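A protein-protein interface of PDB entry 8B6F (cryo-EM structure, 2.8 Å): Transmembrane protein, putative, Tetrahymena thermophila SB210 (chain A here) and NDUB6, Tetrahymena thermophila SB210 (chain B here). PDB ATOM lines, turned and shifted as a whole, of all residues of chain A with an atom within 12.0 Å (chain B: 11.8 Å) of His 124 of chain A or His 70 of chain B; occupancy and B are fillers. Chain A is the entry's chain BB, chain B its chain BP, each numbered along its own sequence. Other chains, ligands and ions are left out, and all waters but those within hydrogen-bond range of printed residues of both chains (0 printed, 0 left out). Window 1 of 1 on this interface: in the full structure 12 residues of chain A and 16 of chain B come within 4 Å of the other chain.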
ATOM      1  N   GLU A 117      13.838 -20.654   1.131  1.00  0.00           N
ATOM      2  CA  GLU A 117      15.122 -20.779   0.455  1.00  0.00           C
ATOM      3  C   GLU A 117      14.986 -20.301  -0.984  1.00  0.00           C
ATOM      4  O   GLU A 117      14.209 -20.863  -1.762  1.00  0.00           O
ATOM      5  CB  GLU A 117      15.602 -22.225   0.499  1.00  0.00           C
ATOM      6  CG  GLU A 117      16.950 -22.449  -0.163  1.00  0.00           C
ATOM      7  CD  GLU A 117      18.076 -21.708   0.527  1.00  0.00           C
ATOM      8  OE1 GLU A 117      17.880 -21.264   1.677  1.00  0.00           O
ATOM      9  OE2 GLU A 117      19.158 -21.569  -0.081  1.00  0.00           O
ATOM     10  N   GLY A 118      15.745 -19.270  -1.338  1.00  0.00           N
ATOM     11  CA  GLY A 118      15.660 -18.670  -2.651  1.00  0.00           C
ATOM     12  C   GLY A 118      16.383 -19.404  -3.752  1.00  0.00           C
ATOM     13  O   GLY A 118      16.295 -18.992  -4.910  1.00  0.00           O
ATOM     14  N   LEU A 119      17.105 -20.479  -3.429  1.00  0.00           N
ATOM     15  CA  LEU A 119      17.845 -21.248  -4.423  1.00  0.00           C
ATOM     16  C   LEU A 119      17.320 -22.668  -4.586  1.00  0.00           C
ATOM     17  O   LEU A 119      17.957 -23.475  -5.272  1.00  0.00           O
ATOM     18  CB  LEU A 119      19.334 -21.273  -4.066  1.00  0.00           C
ATOM     19  CG  LEU A 119      20.069 -19.943  -4.266  1.00  0.00           C
ATOM     20  CD1 LEU A 119      21.447 -19.987  -3.643  1.00  0.00           C
ATOM     21  CD2 LEU A 119      20.175 -19.594  -5.741  1.00  0.00           C
ATOM     22  N   MET A 120      16.186 -23.002  -3.974  1.00  0.00           N
ATOM     23  CA  MET A 120      15.513 -24.258  -4.269  1.00  0.00           C
ATOM     24  C   MET A 120      14.741 -24.112  -5.572  1.00  0.00           C
ATOM     25  O   MET A 120      13.939 -23.187  -5.727  1.00  0.00           O
ATOM     26  CB  MET A 120      14.565 -24.650  -3.137  1.00  0.00           C
ATOM     27  CG  MET A 120      15.252 -25.197  -1.900  1.00  0.00           C
ATOM     28  SD  MET A 120      16.233 -26.681  -2.210  1.00  0.00           S
ATOM     29  CE  MET A 120      15.000 -27.797  -2.866  1.00  0.00           C
ATOM     30  N   ASN A 121      14.981 -25.023  -6.504  1.00  0.00           N
ATOM     31  CA  ASN A 121      14.433 -24.919  -7.846  1.00  0.00           C
ATOM     32  C   ASN A 121      13.170 -25.756  -7.973  1.00  0.00           C
ATOM     33  O   ASN A 121      13.106 -26.886  -7.481  1.00  0.00           O
ATOM     34  CB  ASN A 121      15.459 -25.375  -8.886  1.00  0.00           C
ATOM     35  CG  ASN A 121      16.732 -24.559  -8.843  1.00  0.00           C
ATOM     36  OD1 ASN A 121      16.704 -23.357  -8.593  1.00  0.00           O
ATOM     37  ND2 ASN A 121      17.861 -25.214  -9.080  1.00  0.00           N
ATOM     38  N   GLU A 122      12.167 -25.186  -8.604  1.00  0.00           N
ATOM     39  CA  GLU A 122      11.016 -25.928  -9.079  1.00  0.00           C
ATOM     40  C   GLU A 122      11.295 -26.446 -10.481  1.00  0.00           C
ATOM     41  O   GLU A 122      12.198 -25.952 -11.163  1.00  0.00           O
ATOM     42  CB  GLU A 122       9.778 -25.034  -9.073  1.00  0.00           C
ATOM     43  CG  GLU A 122       9.321 -24.644  -7.680  1.00  0.00           C
ATOM     44  CD  GLU A 122       8.055 -23.813  -7.697  1.00  0.00           C
ATOM     45  OE1 GLU A 122       7.539 -23.543  -8.800  1.00  0.00           O
ATOM     46  OE2 GLU A 122       7.576 -23.430  -6.609  1.00  0.00           O
ATOM     47  N   PRO A 123      10.558 -27.451 -10.947  1.00  0.00           N
ATOM     48  CA  PRO A 123      10.835 -27.991 -12.283  1.00  0.00           C
ATOM     49  C   PRO A 123      10.850 -26.887 -13.328  1.00  0.00           C
ATOM     50  O   PRO A 123       9.963 -26.033 -13.372  1.00  0.00           O
ATOM     51  CB  PRO A 123       9.689 -28.986 -12.511  1.00  0.00           C
ATOM     52  CG  PRO A 123       8.682 -28.698 -11.440  1.00  0.00           C
ATOM     53  CD  PRO A 123       9.459 -28.172 -10.288  1.00  0.00           C
ATOM     54  N   HIS A 124      11.878 -26.902 -14.171  1.00  0.00           N
ATOM     55  CA  HIS A 124      12.096 -25.837 -15.140  1.00  0.00           C
ATOM     56  C   HIS A 124      12.947 -26.388 -16.276  1.00  0.00           C
ATOM     57  O   HIS A 124      13.403 -27.534 -16.243  1.00  0.00           O
ATOM     58  CB  HIS A 124      12.764 -24.622 -14.489  1.00  0.00           C
ATOM     59  CG  HIS A 124      14.149 -24.892 -13.989  1.00  0.00           C
ATOM     60  ND1 HIS A 124      15.228 -25.041 -14.834  1.00  0.00           N
ATOM     61  CD2 HIS A 124      14.632 -25.043 -12.734  1.00  0.00           C
ATOM     62  CE1 HIS A 124      16.315 -25.272 -14.121  1.00  0.00           C
ATOM     63  NE2 HIS A 124      15.980 -25.279 -12.844  1.00  0.00           N
ATOM     64  N   GLY A 125      13.163 -25.553 -17.284  1.00  0.00           N
ATOM     65  CA  GLY A 125      13.945 -25.911 -18.446  1.00  0.00           C
ATOM     66  C   GLY A 125      13.071 -26.323 -19.618  1.00  0.00           C
ATOM     67  O   GLY A 125      11.898 -26.673 -19.472  1.00  0.00           O
ATOM     68  N   TYR A 126      13.664 -26.279 -20.806  1.00  0.00           N
ATOM     69  CA  TYR A 126      12.989 -26.665 -22.038  1.00  0.00           C
ATOM     70  C   TYR A 126      13.351 -28.104 -22.365  1.00  0.00           C
ATOM     71  O   TYR A 126      14.530 -28.470 -22.358  1.00  0.00           O
ATOM     72  CB  TYR A 126      13.377 -25.739 -23.190  1.00  0.00           C
ATOM     73  CG  TYR A 126      13.026 -24.292 -22.939  1.00  0.00           C
ATOM     74  CD1 TYR A 126      11.706 -23.863 -22.972  1.00  0.00           C
ATOM     75  CD2 TYR A 126      14.014 -23.357 -22.668  1.00  0.00           C
ATOM     76  CE1 TYR A 126      11.380 -22.545 -22.741  1.00  0.00           C
ATOM     77  CE2 TYR A 126      13.698 -22.036 -22.436  1.00  0.00           C
ATOM     78  CZ  TYR A 126      12.379 -21.636 -22.473  1.00  0.00           C
ATOM     79  OH  TYR A 126      12.062 -20.319 -22.244  1.00  0.00           O
ATOM     80  N   LEU A 127      12.334 -28.917 -22.653  1.00  0.00           N
ATOM     81  CA  LEU A 127      12.570 -30.337 -22.877  1.00  0.00           C
ATOM     82  C   LEU A 127      13.495 -30.566 -24.064  1.00  0.00           C
ATOM     83  O   LEU A 127      14.403 -31.402 -24.002  1.00  0.00           O
ATOM     84  CB  LEU A 127      11.236 -31.055 -23.089  1.00  0.00           C
ATOM     85  CG  LEU A 127      11.288 -32.580 -23.199  1.00  0.00           C
ATOM     86  CD1 LEU A 127      11.812 -33.204 -21.914  1.00  0.00           C
ATOM     87  CD2 LEU A 127       9.915 -33.133 -23.542  1.00  0.00           C
ATOM     88  N   THR A 128      13.281 -29.832 -25.151  1.00  0.00           N
ATOM     89  CA  THR A 128      14.073 -29.953 -26.366  1.00  0.00           C
ATOM     90  C   THR A 128      14.465 -28.563 -26.847  1.00  0.00           C
ATOM     91  O   THR A 128      14.122 -27.549 -26.236  1.00  0.00           O
ATOM     92  CB  THR A 128      13.304 -30.690 -27.465  1.00  0.00           C
ATOM     93  OG1 THR A 128      12.091 -29.985 -27.736  1.00  0.00           O
ATOM     94  CG2 THR A 128      12.976 -32.111 -27.030  1.00  0.00           C
ATOM     95  N   MET A 129      15.192 -28.523 -27.961  1.00  0.00           N
ATOM     96  CA  MET A 129      15.635 -27.260 -28.534  1.00  0.00           C
ATOM     97  C   MET A 129      14.576 -26.605 -29.412  1.00  0.00           C
ATOM     98  O   MET A 129      14.792 -25.483 -29.878  1.00  0.00           O
ATOM     99  CB  MET A 129      16.912 -27.484 -29.346  1.00  0.00           C
ATOM    100  CG  MET A 129      17.579 -26.205 -29.808  1.00  0.00           C
ATOM    101  SD  MET A 129      19.296 -26.457 -30.290  1.00  0.00           S
ATOM    102  CE  MET A 129      19.107 -27.676 -31.585  1.00  0.00           C
ATOM    103  N   ASP A 130      13.444 -27.266 -29.647  1.00  0.00           N
ATOM    104  CA  ASP A 130      12.390 -26.677 -30.460  1.00  0.00           C
ATOM    105  C   ASP A 130      11.739 -25.506 -29.734  1.00  0.00           C
ATOM    106  O   ASP A 130      11.460 -25.572 -28.535  1.00  0.00           O
ATOM    107  CB  ASP A 130      11.334 -27.724 -30.807  1.00  0.00           C
ATOM    108  CG  ASP A 130      11.850 -28.773 -31.768  1.00  0.00           C
ATOM    109  OD1 ASP A 130      13.081 -28.853 -31.954  1.00  0.00           O
ATOM    110  OD2 ASP A 130      11.025 -29.507 -32.349  1.00  0.00           O
ATOM    111  N   PRO A 132       8.886 -23.316 -28.419  1.00  0.00           N
ATOM    112  CA  PRO A 132       7.448 -23.532 -28.189  1.00  0.00           C
ATOM    113  C   PRO A 132       6.562 -22.689 -29.085  1.00  0.00           C
ATOM    114  O   PRO A 132       5.499 -23.155 -29.512  1.00  0.00           O
ATOM    115  CB  PRO A 132       7.272 -23.160 -26.710  1.00  0.00           C
ATOM    116  CG  PRO A 132       8.611 -23.338 -26.109  1.00  0.00           C
ATOM    117  CD  PRO A 132       9.596 -22.975 -27.174  1.00  0.00           C
ATOM    118  N   TYR B  63      23.839 -22.782  -5.399  1.00  0.00           N
ATOM    119  CA  TYR B  63      24.199 -21.794  -6.399  1.00  0.00           C
ATOM    120  C   TYR B  63      23.128 -21.741  -7.479  1.00  0.00           C
ATOM    121  O   TYR B  63      22.412 -22.723  -7.695  1.00  0.00           O
ATOM    122  CB  TYR B  63      25.558 -22.120  -7.033  1.00  0.00           C
ATOM    123  CG  TYR B  63      25.688 -23.551  -7.494  1.00  0.00           C
ATOM    124  CD1 TYR B  63      25.272 -23.932  -8.761  1.00  0.00           C
ATOM    125  CD2 TYR B  63      26.232 -24.520  -6.664  1.00  0.00           C
ATOM    126  CE1 TYR B  63      25.390 -25.239  -9.188  1.00  0.00           C
ATOM    127  CE2 TYR B  63      26.353 -25.830  -7.081  1.00  0.00           C
ATOM    128  CZ  TYR B  63      25.930 -26.183  -8.344  1.00  0.00           C
ATOM    129  OH  TYR B  63      26.050 -27.485  -8.766  1.00  0.00           O
ATOM    130  N   PRO B  64      22.991 -20.607  -8.165  1.00  0.00           N
ATOM    131  CA  PRO B  64      21.930 -20.483  -9.172  1.00  0.00           C
ATOM    132  C   PRO B  64      22.103 -21.467 -10.320  1.00  0.00           C
ATOM    133  O   PRO B  64      23.218 -21.786 -10.735  1.00  0.00           O
ATOM    134  CB  PRO B  64      22.064 -19.033  -9.654  1.00  0.00           C
ATOM    135  CG  PRO B  64      23.454 -18.643  -9.314  1.00  0.00           C
ATOM    136  CD  PRO B  64      23.789 -19.374  -8.056  1.00  0.00           C
ATOM    137  N   ILE B  65      20.972 -21.939 -10.835  1.00  0.00           N
ATOM    138  CA  ILE B  65      20.924 -22.852 -11.969  1.00  0.00           C
ATOM    139  C   ILE B  65      20.164 -22.149 -13.084  1.00  0.00           C
ATOM    140  O   ILE B  65      19.100 -21.584 -12.828  1.00  0.00           O
ATOM    141  CB  ILE B  65      20.239 -24.187 -11.619  1.00  0.00           C
ATOM    142  CG1 ILE B  65      20.907 -24.837 -10.402  1.00  0.00           C
ATOM    143  CG2 ILE B  65      20.256 -25.129 -12.815  1.00  0.00           C
ATOM    144  CD1 ILE B  65      22.359 -25.213 -10.605  1.00  0.00           C
ATOM    145  N   PRO B  66      20.657 -22.151 -14.324  1.00  0.00           N
ATOM    146  CA  PRO B  66      19.937 -21.447 -15.392  1.00  0.00           C
ATOM    147  C   PRO B  66      18.531 -21.995 -15.578  1.00  0.00           C
ATOM    148  O   PRO B  66      18.298 -23.203 -15.506  1.00  0.00           O
ATOM    149  CB  PRO B  66      20.808 -21.694 -16.630  1.00  0.00           C
ATOM    150  CG  PRO B  66      21.627 -22.885 -16.297  1.00  0.00           C
ATOM    151  CD  PRO B  66      21.873 -22.807 -14.828  1.00  0.00           C
ATOM    152  N   ARG B  67      17.585 -21.086 -15.824  1.00  0.00           N
ATOM    153  CA  ARG B  67      16.194 -21.493 -15.992  1.00  0.00           C
ATOM    154  C   ARG B  67      16.006 -22.330 -17.251  1.00  0.00           C
ATOM    155  O   ARG B  67      15.252 -23.308 -17.247  1.00  0.00           O
ATOM    156  CB  ARG B  67      15.291 -20.260 -16.039  1.00  0.00           C
ATOM    157  CG  ARG B  67      15.304 -19.406 -14.780  1.00  0.00           C
ATOM    158  CD  ARG B  67      14.425 -19.989 -13.686  1.00  0.00           C
ATOM    159  NE  ARG B  67      15.029 -21.151 -13.046  1.00  0.00           N
ATOM    160  CZ  ARG B  67      15.854 -21.096 -12.009  1.00  0.00           C
ATOM    161  NH1 ARG B  67      16.204 -19.944 -11.463  1.00  0.00           N
ATOM    162  NH2 ARG B  67      16.341 -22.226 -11.509  1.00  0.00           N
ATOM    163  N   TYR B  68      16.681 -21.960 -18.340  1.00  0.00           N
ATOM    164  CA  TYR B  68      16.470 -22.640 -19.613  1.00  0.00           C
ATOM    165  C   TYR B  68      16.944 -24.085 -19.590  1.00  0.00           C
ATOM    166  O   TYR B  68      16.490 -24.883 -20.416  1.00  0.00           O
ATOM    167  CB  TYR B  68      17.193 -21.895 -20.736  1.00  0.00           C
ATOM    168  CG  TYR B  68      18.612 -22.369 -20.964  1.00  0.00           C
ATOM    169  CD1 TYR B  68      19.662 -21.877 -20.201  1.00  0.00           C
ATOM    170  CD2 TYR B  68      18.898 -23.307 -21.947  1.00  0.00           C
ATOM    171  CE1 TYR B  68      20.956 -22.309 -20.409  1.00  0.00           C
ATOM    172  CE2 TYR B  68      20.186 -23.743 -22.161  1.00  0.00           C
ATOM    173  CZ  TYR B  68      21.211 -23.242 -21.391  1.00  0.00           C
ATOM    174  OH  TYR B  68      22.495 -23.679 -21.608  1.00  0.00           O
ATOM    175  N   LEU B  69      17.841 -24.438 -18.677  1.00  0.00           N
ATOM    176  CA  LEU B  69      18.463 -25.753 -18.672  1.00  0.00           C
ATOM    177  C   LEU B  69      17.620 -26.727 -17.859  1.00  0.00           C
ATOM    178  O   LEU B  69      17.315 -26.471 -16.691  1.00  0.00           O
ATOM    179  CB  LEU B  69      19.878 -25.663 -18.103  1.00  0.00           C
ATOM    180  CG  LEU B  69      20.788 -26.868 -18.342  1.00  0.00           C
ATOM    181  CD1 LEU B  69      21.028 -27.103 -19.824  1.00  0.00           C
ATOM    182  CD2 LEU B  69      22.105 -26.696 -17.602  1.00  0.00           C
ATOM    183  N   HIS B  70      17.251 -27.845 -18.483  1.00  0.00           N
ATOM    184  CA  HIS B  70      16.412 -28.860 -17.848  1.00  0.00           C
ATOM    185  C   HIS B  70      17.312 -29.813 -17.070  1.00  0.00           C
ATOM    186  O   HIS B  70      17.707 -30.869 -17.562  1.00  0.00           O
ATOM    187  CB  HIS B  70      15.588 -29.592 -18.897  1.00  0.00           C
ATOM    188  CG  HIS B  70      14.506 -30.453 -18.326  1.00  0.00           C
ATOM    189  ND1 HIS B  70      13.807 -31.367 -19.084  1.00  0.00           N
ATOM    190  CD2 HIS B  70      14.006 -30.543 -17.072  1.00  0.00           C
ATOM    191  CE1 HIS B  70      12.920 -31.980 -18.322  1.00  0.00           C
ATOM    192  NE2 HIS B  70      13.021 -31.498 -17.097  1.00  0.00           N
ATOM    193  N   VAL B  71      17.637 -29.432 -15.833  1.00  0.00           N
ATOM    194  CA  VAL B  71      18.524 -30.200 -14.973  1.00  0.00           C
ATOM    195  C   VAL B  71      17.864 -30.397 -13.615  1.00  0.00           C
ATOM    196  O   VAL B  71      16.932 -29.684 -13.240  1.00  0.00           O
ATOM    197  CB  VAL B  71      19.903 -29.530 -14.808  1.00  0.00           C
ATOM    198  CG1 VAL B  71      20.714 -29.707 -16.070  1.00  0.00           C
ATOM    199  CG2 VAL B  71      19.745 -28.055 -14.467  1.00  0.00           C
ATOM    200  N   GLY B  72      18.362 -31.387 -12.882  1.00  0.00           N
ATOM    201  CA  GLY B  72      17.787 -31.807 -11.623  1.00  0.00           C
ATOM    202  C   GLY B  72      18.389 -31.190 -10.378  1.00  0.00           C
ATOM    203  O   GLY B  72      18.064 -31.635  -9.273  1.00  0.00           O
ATOM    204  N   GLN B  73      19.250 -30.182 -10.508  1.00  0.00           N
ATOM    205  CA  GLN B  73      19.883 -29.583  -9.338  1.00  0.00           C
ATOM    206  C   GLN B  73      18.850 -28.941  -8.422  1.00  0.00           C
ATOM    207  O   GLN B  73      18.243 -27.927  -8.777  1.00  0.00           O
ATOM    208  CB  GLN B  73      20.924 -28.542  -9.757  1.00  0.00           C
ATOM    209  CG  GLN B  73      22.241 -29.119 -10.255  1.00  0.00           C
ATOM    210  CD  GLN B  73      22.097 -29.871 -11.558  1.00  0.00           C
ATOM    211  OE1 GLN B  73      21.050 -30.451 -11.842  1.00  0.00           O
ATOM    212  NE2 GLN B  73      23.150 -29.861 -12.366  1.00  0.00           N
ATOM    213  N   TRP B  74      18.658 -29.517  -7.236  1.00  0.00           N
ATOM    214  CA  TRP B  74      17.761 -28.964  -6.222  1.00  0.00           C
ATOM    215  C   TRP B  74      16.356 -28.740  -6.777  1.00  0.00           C
ATOM    216  O   TRP B  74      15.752 -27.681  -6.597  1.00  0.00           O
ATOM    217  CB  TRP B  74      18.326 -27.665  -5.650  1.00  0.00           C
ATOM    218  CG  TRP B  74      19.519 -27.854  -4.771  1.00  0.00           C
ATOM    219  CD1 TRP B  74      19.545 -28.453  -3.548  1.00  0.00           C
ATOM    220  CD2 TRP B  74      20.860 -27.431  -5.041  1.00  0.00           C
ATOM    221  NE1 TRP B  74      20.818 -28.433  -3.039  1.00  0.00           N
ATOM    222  CE2 TRP B  74      21.646 -27.814  -3.937  1.00  0.00           C
ATOM    223  CE3 TRP B  74      21.472 -26.771  -6.109  1.00  0.00           C
ATOM    224  CZ2 TRP B  74      23.012 -27.554  -3.869  1.00  0.00           C
ATOM    225  CZ3 TRP B  74      22.829 -26.516  -6.042  1.00  0.00           C
ATOM    226  CH2 TRP B  74      23.585 -26.907  -4.930  1.00  0.00           C
ATOM    227  N   ILE B  75      15.828 -29.754  -7.453  1.00  0.00           N
ATOM    228  CA  ILE B  75      14.479 -29.697  -8.007  1.00  0.00           C
ATOM    229  C   ILE B  75      13.507 -30.252  -6.976  1.00  0.00           C
ATOM    230  O   ILE B  75      13.666 -31.382  -6.502  1.00  0.00           O
ATOM    231  CB  ILE B  75      14.383 -30.469  -9.332  1.00  0.00           C
ATOM    232  CG1 ILE B  75      15.120 -29.726 -10.451  1.00  0.00           C
ATOM    233  CG2 ILE B  75      12.923 -30.708  -9.723  1.00  0.00           C
ATOM    234  CD1 ILE B  75      14.531 -28.376 -10.822  1.00  0.00           C
ATOM    235  N   VAL B  76      12.501 -29.454  -6.626  1.00  0.00           N
ATOM    236  CA  VAL B  76      11.427 -29.864  -5.731  1.00  0.00           C
ATOM    237  C   VAL B  76      10.110 -29.453  -6.371  1.00  0.00           C
ATOM    238  O   VAL B  76       9.959 -28.306  -6.805  1.00  0.00           O
ATOM    239  CB  VAL B  76      11.579 -29.240  -4.329  1.00  0.00           C
ATOM    240  CG1 VAL B  76      11.835 -27.748  -4.437  1.00  0.00           C
ATOM    241  CG2 VAL B  76      10.349 -29.514  -3.474  1.00  0.00           C
ATOM    242  N   ASN B  77       9.163 -30.384  -6.434  1.00  0.00           N
ATOM    243  CA  ASN B  77       7.888 -30.174  -7.106  1.00  0.00           C
ATOM    244  C   ASN B  77       6.792 -29.986  -6.066  1.00  0.00           C
ATOM    245  O   ASN B  77       6.710 -30.750  -5.100  1.00  0.00           O
ATOM    246  CB  ASN B  77       7.557 -31.355  -8.021  1.00  0.00           C
ATOM    247  CG  ASN B  77       6.407 -31.063  -8.961  1.00  0.00           C
ATOM    248  OD1 ASN B  77       5.499 -30.300  -8.635  1.00  0.00           O
ATOM    249  ND2 ASN B  77       6.440 -31.671 -10.140  1.00  0.00           N
ATOM    250  N   LYS B  78       5.958 -28.963  -6.268  1.00  0.00           N
ATOM    251  CA  LYS B  78       4.870 -28.688  -5.336  1.00  0.00           C
ATOM    252  C   LYS B  78       3.822 -29.793  -5.356  1.00  0.00           C
ATOM    253  O   LYS B  78       3.267 -30.150  -4.311  1.00  0.00           O
ATOM    254  CB  LYS B  78       4.224 -27.344  -5.670  1.00  0.00           C
ATOM    255  CG  LYS B  78       5.061 -26.136  -5.292  1.00  0.00           C
ATOM    256  CD  LYS B  78       5.094 -25.950  -3.787  1.00  0.00           C
ATOM    257  CE  LYS B  78       5.547 -24.549  -3.417  1.00  0.00           C
ATOM    258  NZ  LYS B  78       5.514 -24.330  -1.942  1.00  0.00           N
ATOM    259  N   ASN B  83       1.600 -36.405  -8.046  1.00  0.00           N
ATOM    260  CA  ASN B  83       2.474 -37.064  -9.010  1.00  0.00           C
ATOM    261  C   ASN B  83       2.819 -38.473  -8.550  1.00  0.00           C
ATOM    262  O   ASN B  83       2.778 -39.421  -9.340  1.00  0.00           O
ATOM    263  CB  ASN B  83       3.742 -36.239  -9.226  1.00  0.00           C
ATOM    264  CG  ASN B  83       3.456 -34.875  -9.817  1.00  0.00           C
ATOM    265  OD1 ASN B  83       2.404 -34.655 -10.412  1.00  0.00           O
ATOM    266  ND2 ASN B  83       4.400 -33.956  -9.668  1.00  0.00           N
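The guanidinium group of Arg 67 of chain B is in hydrogen-bond range of the side-chain amide oxygen of Asn 121 of chain A (3.1 Å). The side-chain amide nitrogen of Asn 121 of chain A sits at hydrogen-bond distance from the backbone carbonyl oxygen of Gln 73 of chain B, at 2.8 Å. The backbone NH of Asn 121 of chain A lies within hydrogen-bond range of the backbone carbonyl oxygen of Trp 74 of chain B, at 2.8 Å. The backbone NH (N) of Val 76 of chain B is in hydrogen-bond range of the backbone carbonyl oxygen (O) of Asn 121 of chain A, 2.8 Å away. A ring nitrogen (ND1) of His 124 of chain A sits at hydrogen-bond distance from the backbone carbonyl oxygen of Arg 67 of chain B, 3.0 Å away. A ring nitrogen (ND1) of His 124 of chain A sits close to the backbone carbonyl oxygen (O) of Leu 69 of chain B, 3.1 Å away. O of Arg 67 of chain B is in hydrogen-bond range of N of Gly 125 of chain A (3.1 Å). N of Tyr 126 of chain A sits at hydrogen-bond distance from O of Tyr 68 of chain B, 3.2 Å away.
The backbone carbonyl oxygen of Ile 65 of chain B lies within hydrogen-bond range of the guanidinium group of Arg 67 of chain B (3.1 Å). The side-chain amide nitrogen of Asn 83 of chain B sits close to the side-chain amide nitrogen of Asn 77 of chain B (3.1 Å).
Among the printed residues, pairs that only touch across the chains: Leu 119 of chain A with Pro 64 of chain B (3.9 Å), Met 120 of chain A with Trp 74 of chain B (3.8 Å), Met 120 of chain A with Val 76 of chain B (3.5 Å), Asn 121 of chain A with Ile 65 of chain B (3.3 Å), Asn 121 of chain A with Ile 75 of chain B (3.2 Å), Glu 122 of chain A with Ile 75 of chain B (3.4 Å), Glu 122 of chain A with Val 76 of chain B (3.5 Å), Glu 122 of chain A with Lys 78 of chain B (3.9 Å), Pro 123 of chain A with Ile 75 of chain B (3.99 Å), Pro 123 of chain A with Val 76 of chain B (3.5 Å), Pro 123 of chain A with Asn 77 of chain B (3.9 Å), His 124 of chain A with Pro 66 of chain B (3.2 Å), His 124 of chain A with His 70 of chain B (3.2 Å), His 124 of chain A with Ile 75 of chain B (3.8 Å), Gly 125 of chain A with Tyr 68 of chain B (3.4 Å), Gly 125 of chain A with Leu 69 of chain B (3.8 Å), Gly 125 of chain A with His 70 of chain B (3.8 Å), Tyr 126 of chain A with His 70 of chain B (3.8 Å) and Leu 127 of chain A with His 70 of chain B (3.9 Å).
Printed residues of chain B within 4 Å of Leu 119 of chain A: Pro 64. Of the printed residues of chain B, Met 120 of chain A touches Trp 74 and Val 76. Of the printed residues of chain B, Pro 123 of chain A touches Ile 75 (3.99 Å), Val 76 (3.5 Å) and Asn 77 (3.9 Å). Of chain B, only Pro 66 (3.2 Å), Arg 67 (3.0 Å), Leu 69 (3.0 Å), His 70 (3.2 Å) and Ile 75 (3.8 Å) come within 4 Å of His 124 of chain A. Leu 127 of chain A touches just one residue of chain B: His 70. Pro 132 of chain A touches none of the printed residues of chain B. Ile 65 of chain B touches one residue of chain A. Tyr 68 of chain B touches two residues of chain A. Printed residues of chain A within 4 Å of Leu 69 of chain B: His 124 (3.0 Å) and Gly 125 (3.8 Å). His 70 of chain B touches just these residues of chain A: His 124, Gly 125, Tyr 126 and Leu 127. Gly 72 of chain B touches none of the printed residues of chain A. Gln 73 of chain B touches just one residue of chain A: Asn 121 (2.8 Å).
Printed residues of chain B that touch a printed residue of chain A: Pro 64, Ile 65, Pro 66, Arg 67, Tyr 68, Leu 69, His 70, Gln 73, Trp 74, Ile 75, Val 76, Asn 77 and Lys 78. Of the 15 printed residues of chain A, 9 touch a printed residue of chain B. Printed residues of chain A that touch a printed residue of chain B: Leu 119, Met 120, Asn 121, Glu 122, Pro 123, His 124, Gly 125, Tyr 126 and Leu 127. Among the printed residues, 27 pairs touch across the chains. Among the printed residues, no Asp or Glu carboxylate lies within 4 Å of a Lys or Arg side-chain nitrogen of the other chain.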
